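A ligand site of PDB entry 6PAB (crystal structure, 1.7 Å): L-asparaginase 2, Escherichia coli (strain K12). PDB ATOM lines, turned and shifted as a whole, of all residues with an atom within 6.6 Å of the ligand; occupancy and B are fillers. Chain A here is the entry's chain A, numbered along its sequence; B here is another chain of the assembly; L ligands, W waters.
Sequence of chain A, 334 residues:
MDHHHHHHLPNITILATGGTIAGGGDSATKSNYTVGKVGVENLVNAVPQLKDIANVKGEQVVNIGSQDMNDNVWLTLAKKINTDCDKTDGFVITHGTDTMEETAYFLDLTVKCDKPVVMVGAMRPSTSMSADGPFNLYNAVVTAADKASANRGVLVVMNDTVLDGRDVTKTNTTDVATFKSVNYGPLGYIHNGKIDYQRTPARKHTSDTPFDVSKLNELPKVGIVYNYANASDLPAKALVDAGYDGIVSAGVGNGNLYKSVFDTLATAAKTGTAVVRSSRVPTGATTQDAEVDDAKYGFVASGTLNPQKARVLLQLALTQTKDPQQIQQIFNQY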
ATOM      1  N   GLY A  18      13.855  18.058  -5.949  1.00  0.00           N
ATOM      2  CA  GLY A  18      13.329  17.002  -5.079  1.00  0.00           C
ATOM      3  C   GLY A  18      11.793  16.952  -4.954  1.00  0.00           C
ATOM      4  O   GLY A  18      11.081  17.047  -5.994  1.00  0.00           O
ATOM      5  N   GLY A  19      11.323  16.737  -3.743  1.00  0.00           N
ATOM      6  CA  GLY A  19       9.880  16.657  -3.503  1.00  0.00           C
ATOM      7  C   GLY A  19       9.241  15.316  -3.690  1.00  0.00           C
ATOM      8  O   GLY A  19       9.855  14.363  -4.180  1.00  0.00           O
ATOM      9  N   THR A  20       7.972  15.216  -3.279  1.00  0.00           N
ATOM     10  CA  THR A  20       7.158  14.027  -3.491  1.00  0.00           C
ATOM     11  C   THR A  20       7.005  13.704  -4.983  1.00  0.00           C
ATOM     12  O   THR A  20       6.857  12.520  -5.338  1.00  0.00           O
ATOM     13  CB  THR A  20       5.850  14.154  -2.774  1.00  0.00           C
ATOM     14  OG1 THR A  20       6.141  14.240  -1.376  1.00  0.00           O
ATOM     15  CG2 THR A  20       4.874  12.975  -2.943  1.00  0.00           C
ATOM     16  N   ILE A  21       7.094  14.725  -5.846  1.00  0.00           N
ATOM     17  CA  ILE A  21       7.121  14.503  -7.280  1.00  0.00           C
ATOM     18  C   ILE A  21       8.248  13.496  -7.657  1.00  0.00           C
ATOM     19  O   ILE A  21       8.072  12.671  -8.594  1.00  0.00           O
ATOM     20  CB  ILE A  21       7.218  15.778  -8.088  1.00  0.00           C
ATOM     21  CG1 ILE A  21       6.935  15.465  -9.614  1.00  0.00           C
ATOM     22  CG2 ILE A  21       8.471  16.578  -7.788  1.00  0.00           C
ATOM     23  CD1 ILE A  21       6.673  16.679 -10.435  1.00  0.00           C
ATOM     24  N   TYR A  33       6.260   6.648   2.123  1.00  0.00           N
ATOM     25  CA  TYR A  33       7.256   6.861   1.076  1.00  0.00           C
ATOM     26  C   TYR A  33       8.401   7.722   1.564  1.00  0.00           C
ATOM     27  O   TYR A  33       8.326   8.351   2.634  1.00  0.00           O
ATOM     28  CB  TYR A  33       6.611   7.505  -0.153  1.00  0.00           C
ATOM     29  CG  TYR A  33       6.209   8.958  -0.001  1.00  0.00           C
ATOM     30  CD1 TYR A  33       4.990   9.311   0.565  1.00  0.00           C
ATOM     31  CD2 TYR A  33       7.065   9.974  -0.380  1.00  0.00           C
ATOM     32  CE1 TYR A  33       4.611  10.641   0.731  1.00  0.00           C
ATOM     33  CE2 TYR A  33       6.702  11.327  -0.210  1.00  0.00           C
ATOM     34  CZ  TYR A  33       5.472  11.663   0.346  1.00  0.00           C
ATOM     35  OH  TYR A  33       5.077  12.987   0.511  1.00  0.00           O
ATOM     36  N   VAL A  35      11.053  10.848   0.227  1.00  0.00           N
ATOM     37  CA  VAL A  35      11.010  12.013  -0.638  1.00  0.00           C
ATOM     38  C   VAL A  35      12.330  12.097  -1.377  1.00  0.00           C
ATOM     39  O   VAL A  35      13.355  11.653  -0.844  1.00  0.00           O
ATOM     40  CB  VAL A  35      10.728  13.286   0.247  1.00  0.00           C
ATOM     41  CG1 VAL A  35      11.966  13.756   1.031  1.00  0.00           C
ATOM     42  CG2 VAL A  35      10.189  14.434  -0.583  1.00  0.00           C
ATOM     43  N   GLY A  36      12.304  12.773  -2.555  1.00  0.00           N
ATOM     44  CA  GLY A  36      13.500  13.344  -3.195  1.00  0.00           C
ATOM     45  C   GLY A  36      14.508  12.228  -3.464  1.00  0.00           C
ATOM     46  O   GLY A  36      15.680  12.322  -3.074  1.00  0.00           O
ATOM     47  N   ILE A  64      15.980  17.066  -2.443  1.00  0.00           N
ATOM     48  CA  ILE A  64      15.571  17.121  -1.023  1.00  0.00           C
ATOM     49  C   ILE A  64      14.058  17.175  -0.883  1.00  0.00           C
ATOM     50  O   ILE A  64      13.301  17.552  -1.810  1.00  0.00           O
ATOM     51  CB  ILE A  64      16.189  18.333  -0.283  1.00  0.00           C
ATOM     52  CG1 ILE A  64      15.833  19.702  -0.917  1.00  0.00           C
ATOM     53  CG2 ILE A  64      17.729  18.261  -0.323  1.00  0.00           C
ATOM     54  CD1 ILE A  64      16.319  20.862  -0.148  1.00  0.00           C
ATOM     55  N   GLY A  65      13.588  16.786   0.284  1.00  0.00           N
ATOM     56  CA  GLY A  65      12.248  17.184   0.663  1.00  0.00           C
ATOM     57  C   GLY A  65      12.203  18.697   0.842  1.00  0.00           C
ATOM     58  O   GLY A  65      13.093  19.269   1.471  1.00  0.00           O
ATOM     59  N   SER A  66      11.118  19.383   0.416  1.00  0.00           N
ATOM     60  CA  SER A  66      11.068  20.838   0.545  1.00  0.00           C
ATOM     61  C   SER A  66      10.789  21.257   2.012  1.00  0.00           C
ATOM     62  O   SER A  66      10.905  22.449   2.351  1.00  0.00           O
ATOM     63  CB  SER A  66      10.057  21.448  -0.409  1.00  0.00           C
ATOM     64  OG  SER A  66       8.727  21.344   0.070  1.00  0.00           O
ATOM     65  N   GLN A  67      10.494  20.290   2.885  1.00  0.00           N
ATOM     66  CA  GLN A  67      10.510  20.590   4.353  1.00  0.00           C
ATOM     67  C   GLN A  67      11.883  21.008   4.831  1.00  0.00           C
ATOM     68  O   GLN A  67      11.973  21.686   5.859  1.00  0.00           O
ATOM     69  CB  GLN A  67       9.956  19.406   5.212  1.00  0.00           C
ATOM     70  CG  GLN A  67      10.801  18.113   5.175  1.00  0.00           C
ATOM     71  CD  GLN A  67      10.276  17.158   4.124  1.00  0.00           C
ATOM     72  OE1 GLN A  67       9.994  17.549   2.959  1.00  0.00           O
ATOM     73  NE2 GLN A  67      10.033  15.901   4.547  1.00  0.00           N
ATOM     74  N   HIS A  95       9.745  20.543  -7.426  1.00  0.00           N
ATOM     75  CA  HIS A  95       9.940  20.950  -6.042  1.00  0.00           C
ATOM     76  C   HIS A  95       8.935  20.273  -5.149  1.00  0.00           C
ATOM     77  O   HIS A  95       7.848  19.899  -5.570  1.00  0.00           O
ATOM     78  CB  HIS A  95       9.885  22.495  -6.066  1.00  0.00           C
ATOM     79  CG  HIS A  95      10.211  23.236  -4.782  1.00  0.00           C
ATOM     80  ND1 HIS A  95       9.425  23.184  -3.652  1.00  0.00           N
ATOM     81  CD2 HIS A  95      11.211  24.110  -4.500  1.00  0.00           C
ATOM     82  CE1 HIS A  95       9.894  24.031  -2.761  1.00  0.00           C
ATOM     83  NE2 HIS A  95      10.999  24.583  -3.222  1.00  0.00           N
ATOM     84  N   GLY A  96       9.296  20.098  -3.888  1.00  0.00           N
ATOM     85  CA  GLY A  96       8.318  19.598  -2.913  1.00  0.00           C
ATOM     86  C   GLY A  96       7.174  20.591  -2.746  1.00  0.00           C
ATOM     87  O   GLY A  96       7.316  21.851  -2.975  1.00  0.00           O
ATOM     88  N   THR A  97       6.038  20.052  -2.392  1.00  0.00           N
ATOM     89  CA  THR A  97       4.851  20.947  -2.197  1.00  0.00           C
ATOM     90  C   THR A  97       4.865  21.729  -0.895  1.00  0.00           C
ATOM     91  O   THR A  97       4.292  22.816  -0.807  1.00  0.00           O
ATOM     92  CB  THR A  97       3.547  20.171  -2.325  1.00  0.00           C
ATOM     93  OG1 THR A  97       3.456  19.192  -1.286  1.00  0.00           O
ATOM     94  CG2 THR A  97       3.419  19.510  -3.710  1.00  0.00           C
ATOM     95  N   ASP A  98       5.549  21.206   0.117  1.00  0.00           N
ATOM     96  CA  ASP A  98       5.447  21.749   1.452  1.00  0.00           C
ATOM     97  C   ASP A  98       5.860  23.228   1.495  1.00  0.00           C
ATOM     98  O   ASP A  98       5.170  23.976   2.119  1.00  0.00           O
ATOM     99  CB  ASP A  98       6.234  20.933   2.496  1.00  0.00           C
ATOM    100  CG  ASP A  98       5.659  19.557   2.715  1.00  0.00           C
ATOM    101  OD1 ASP A  98       4.544  19.268   2.217  1.00  0.00           O
ATOM    102  OD2 ASP A  98       6.340  18.731   3.373  1.00  0.00           O
ATOM    103  N   THR A  99       6.990  23.631   0.887  1.00  0.00           N
ATOM    104  CA  THR A  99       7.446  25.032   0.907  1.00  0.00           C
ATOM    105  C   THR A  99       7.488  25.676  -0.471  1.00  0.00           C
ATOM    106  O   THR A  99       8.072  26.710  -0.662  1.00  0.00           O
ATOM    107  CB  THR A  99       8.809  25.142   1.602  1.00  0.00           C
ATOM    108  OG1 THR A  99       9.799  24.377   0.864  1.00  0.00           O
ATOM    109  CG2 THR A  99       8.670  24.655   3.017  1.00  0.00           C
ATOM    110  N   MET A 100       6.835  25.024  -1.447  1.00  0.00           N
ATOM    111  CA  MET A 100       6.791  25.577  -2.806  1.00  0.00           C
ATOM    112  C   MET A 100       6.282  27.026  -2.817  1.00  0.00           C
ATOM    113  O   MET A 100       6.762  27.849  -3.548  1.00  0.00           O
ATOM    114  CB  MET A 100       5.868  24.724  -3.702  1.00  0.00           C
ATOM    115  CG  MET A 100       5.937  25.216  -5.162  1.00  0.00           C
ATOM    116  SD  MET A 100       5.646  24.012  -6.419  1.00  0.00           S
ATOM    117  CE  MET A 100       4.083  23.321  -5.929  1.00  0.00           C
ATOM    118  N   GLY A 121       4.975  20.534  -8.506  1.00  0.00           N
ATOM    119  CA  GLY A 121       5.189  19.421  -7.575  1.00  0.00           C
ATOM    120  C   GLY A 121       4.157  18.339  -7.778  1.00  0.00           C
ATOM    121  O   GLY A 121       3.410  18.344  -8.760  1.00  0.00           O
ATOM    122  N   ALA A 122       4.044  17.435  -6.787  1.00  0.00           N
ATOM    123  CA  ALA A 122       3.034  16.340  -6.805  1.00  0.00           C
ATOM    124  C   ALA A 122       2.666  15.999  -5.412  1.00  0.00           C
ATOM    125  O   ALA A 122       3.559  15.963  -4.541  1.00  0.00           O
ATOM    126  CB  ALA A 122       3.556  15.105  -7.508  1.00  0.00           C
ATOM    127  N   MET A 123       1.373  15.836  -5.153  1.00  0.00           N
ATOM    128  CA  MET A 123       0.941  15.492  -3.793  1.00  0.00           C
ATOM    129  C   MET A 123       1.047  13.991  -3.518  1.00  0.00           C
ATOM    130  O   MET A 123       1.023  13.580  -2.366  1.00  0.00           O
ATOM    131  CB  MET A 123      -0.493  15.990  -3.570  1.00  0.00           C
ATOM    132  CG  MET A 123      -0.539  17.504  -3.441  1.00  0.00           C
ATOM    133  SD  MET A 123       0.275  18.065  -1.967  1.00  0.00           S
ATOM    134  CE  MET A 123      -0.976  17.599  -0.788  1.00  0.00           C
ATOM    135  N   ARG A 124       1.066  13.191  -4.584  1.00  0.00           N
ATOM    136  CA  ARG A 124       1.267  11.731  -4.477  1.00  0.00           C
ATOM    137  C   ARG A 124       2.668  11.341  -5.002  1.00  0.00           C
ATOM    138  O   ARG A 124       3.176  11.919  -6.000  1.00  0.00           O
ATOM    139  CB  ARG A 124       0.190  10.983  -5.253  1.00  0.00           C
ATOM    140  CG  ARG A 124      -1.194  11.293  -4.738  1.00  0.00           C
ATOM    141  CD  ARG A 124      -2.196  10.753  -5.712  1.00  0.00           C
ATOM    142  NE  ARG A 124      -3.568  10.998  -5.326  1.00  0.00           N
ATOM    143  CZ  ARG A 124      -4.628  10.858  -6.115  1.00  0.00           C
ATOM    144  NH1 ARG A 124      -4.497  10.514  -7.409  1.00  0.00           N
ATOM    145  NH2 ARG A 124      -5.843  11.096  -5.607  1.00  0.00           N
ATOM    146  N   LYS A 170      -0.562  26.453  -0.061  1.00  0.00           N
ATOM    147  CA  LYS A 170      -1.012  25.084   0.123  1.00  0.00           C
ATOM    148  C   LYS A 170      -2.179  25.049   1.127  1.00  0.00           C
ATOM    149  O   LYS A 170      -1.949  25.306   2.272  1.00  0.00           O
ATOM    150  CB  LYS A 170       0.178  24.178   0.598  1.00  0.00           C
ATOM    151  CG  LYS A 170      -0.150  22.688   0.737  1.00  0.00           C
ATOM    152  CD  LYS A 170       1.099  21.813   0.891  1.00  0.00           C
ATOM    153  CE  LYS A 170       0.716  20.370   0.976  1.00  0.00           C
ATOM    154  NZ  LYS A 170       1.897  19.476   0.945  1.00  0.00           N
ATOM    155  N   VAL B 252       5.004  21.772   8.044  1.00  0.00           N
ATOM    156  CA  VAL B 252       4.726  22.127   6.661  1.00  0.00           C
ATOM    157  C   VAL B 252       4.000  20.911   6.036  1.00  0.00           C
ATOM    158  O   VAL B 252       4.307  19.735   6.335  1.00  0.00           O
ATOM    159  CB  VAL B 252       6.009  22.584   5.875  1.00  0.00           C
ATOM    160  CG1 VAL B 252       6.538  23.831   6.508  1.00  0.00           C
ATOM    161  CG2 VAL B 252       7.076  21.509   5.793  1.00  0.00           C
ATOM    162  N   GLY B 253       3.102  21.156   5.076  1.00  0.00           N
ATOM    163  CA  GLY B 253       2.390  20.064   4.482  1.00  0.00           C
ATOM    164  C   GLY B 253       1.733  19.095   5.471  1.00  0.00           C
ATOM    165  O   GLY B 253       1.062  19.498   6.472  1.00  0.00           O
ATOM    166  N   ASN B 254       1.900  17.798   5.205  1.00  0.00           N
ATOM    167  CA  ASN B 254       1.342  16.750   6.046  1.00  0.00           C
ATOM    168  C   ASN B 254       2.192  16.596   7.335  1.00  0.00           C
ATOM    169  O   ASN B 254       2.850  15.547   7.549  1.00  0.00           O
ATOM    170  CB  ASN B 254       1.247  15.453   5.258  1.00  0.00           C
ATOM    171  CG  ASN B 254       0.431  14.408   5.964  1.00  0.00           C
ATOM    172  OD1 ASN B 254       0.112  14.520   7.133  1.00  0.00           O
ATOM    173  ND2 ASN B 254       0.159  13.293   5.234  1.00  0.00           N
ATOM    174  N   ASN B 256       5.074  17.890   8.315  1.00  0.00           N
ATOM    175  CA  ASN B 256       6.529  17.752   8.190  1.00  0.00           C
ATOM    176  C   ASN B 256       7.309  18.813   8.898  1.00  0.00           C
ATOM    177  O   ASN B 256       6.852  19.971   9.166  1.00  0.00           O
ATOM    178  CB  ASN B 256       6.937  17.556   6.730  1.00  0.00           C
ATOM    179  CG  ASN B 256       6.372  16.253   6.159  1.00  0.00           C
ATOM    180  OD1 ASN B 256       6.575  15.144   6.705  1.00  0.00           O
ATOM    181  ND2 ASN B 256       5.600  16.389   5.021  1.00  0.00           N
ATOM    182  N   GLU B 291       5.673  10.467   5.628  1.00  0.00           N
ATOM    183  CA  GLU B 291       7.113  10.512   5.612  1.00  0.00           C
ATOM    184  C   GLU B 291       7.735  10.287   6.973  1.00  0.00           C
ATOM    185  O   GLU B 291       8.931  10.062   7.044  1.00  0.00           O
ATOM    186  CB  GLU B 291       7.614  11.834   5.032  1.00  0.00           C
ATOM    187  CG  GLU B 291       7.243  12.058   3.570  1.00  0.00           C
ATOM    188  CD  GLU B 291       7.599  13.480   3.145  1.00  0.00           C
ATOM    189  OE1 GLU B 291       8.851  13.733   3.038  1.00  0.00           O
ATOM    190  OE2 GLU B 291       6.673  14.279   2.942  1.00  0.00           O
HETATM  191  N1  LIG L   1       7.434  16.616   1.965  1.00  0.00           N
HETATM  192  C1  LIG L   1       7.199  16.652   0.493  1.00  0.00           C
HETATM  193  C2  LIG L   1       8.014  17.841   0.027  1.00  0.00           C
HETATM  194  O1  LIG L   1       7.550  19.009   0.218  1.00  0.00           O
HETATM  195  C3  LIG L   1       5.665  16.783   0.206  1.00  0.00           C
HETATM  196  C4  LIG L   1       5.326  16.912  -1.238  1.00  0.00           C
HETATM  197  O2  LIG L   1       4.128  16.656  -1.592  1.00  0.00           O
HETATM  198  O3  LIG L   1       6.219  17.210  -2.051  1.00  0.00           O
HETATM  199  O4  LIG L   1       9.165  17.671  -0.518  1.00  0.00           O
HETATM  200  O   HOH W   1       6.326  17.551  -4.957  1.00  0.00           O
HETATM  201  O   HOH W   2       2.381  15.026  -0.384  1.00  0.00           O
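The side-chain hydroxyl of Ser 66 sits at hydrogen-bond distance from an oxygen (O1) of the ligand.
A nitrogen (N1) of the ligand is in salt-bridge range of the side-chain carboxylate (OE2) of Glu 291 of chain B, at 2.6 Å.
The side-chain hydroxyl (OG1) of Thr 20 lies close to an oxygen (O3) of the ligand, at 3.0 Å.
The backbone carbonyl oxygen of Ala 122 sits close to an oxygen (O2) of the ligand.
The backbone NH (N) of Asp 98 lies within hydrogen-bond range of an oxygen (O1) of the ligand (3.0 Å).
The side-chain hydroxyl (OG1) of Thr 97 sits at hydrogen-bond distance from an oxygen (O2) of the ligand (2.6 Å).
N of Thr 97 is in hydrogen-bond range of O3 of the ligand (2.9 Å).
The backbone NH (N) of Ser 66 lies within hydrogen-bond range of an oxygen (O4) of the ligand, 2.8 Å away.
A nitrogen (N1) of the ligand is in hydrogen-bond range of the side-chain amide oxygen (OE1) of Gln 67, at 2.9 Å.
The backbone NH (N) of Thr 20 is in hydrogen-bond range of an oxygen (O3) of the ligand.
OD2 of Asp 98 is in salt-bridge range of N1 of the ligand (2.8 Å).
OG of Ser 66 is in hydrogen-bond range of N of Asp 98 (3.2 Å).
OD2 of Asp 98 lies within hydrogen-bond range of ND2 of Asn 256 of chain B.
The side-chain carboxylate of Asp 98 is in salt-bridge range of the side-chain amino group of Lys 170.
The side-chain hydroxyl of Thr 97 lies within hydrogen-bond range of the side-chain sulfur of Met 123 (3.4 Å).
The backbone carbonyl oxygen of Ile 64 lies within hydrogen-bond range of the backbone NH of Gly 19 (2.9 Å).
The side-chain hydroxyl of Thr 20 lies within hydrogen-bond range of the side-chain hydroxyl of Tyr 33, at 2.5 Å.
The side-chain hydroxyl of Thr 97 sits at hydrogen-bond distance from the side-chain amino group of Lys 170 (2.7 Å).
The side-chain carboxylate (OE2) of Glu 291 of chain B lies within hydrogen-bond range of the side-chain hydroxyl (OH) of Tyr 33 (3.2 Å).
CA of Gly 19 touches O4 of the ligand, 3.2 Å away.
Tyr 33 touches the ligand.
Val 35 touches the ligand.
Gly 65 touches the ligand (CA to O4, 3.3 Å).
CA of Gly 96 touches O4 of the ligand, 3.2 Å away.
ND2 of Asn 256 of chain B touches N1 of the ligand, 3.6 Å away.
Within 4 Å of the ligand: Gly 19, Thr 20, Tyr 33, Val 35, Gly 65, Ser 66, Gln 67, Gly 96, Thr 97, Asp 98, Ala 122, Asn 256 of chain B and Glu 291 of chain B.
The nearest printed residue that does not touch the ligand is Met 123 (4.04 Å).
Water W2 lies within hydrogen-bond range of O2 of the ligand (2.7 Å), O of Met 123 (2.8 Å) and OH of Tyr 33 (3.5 Å).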
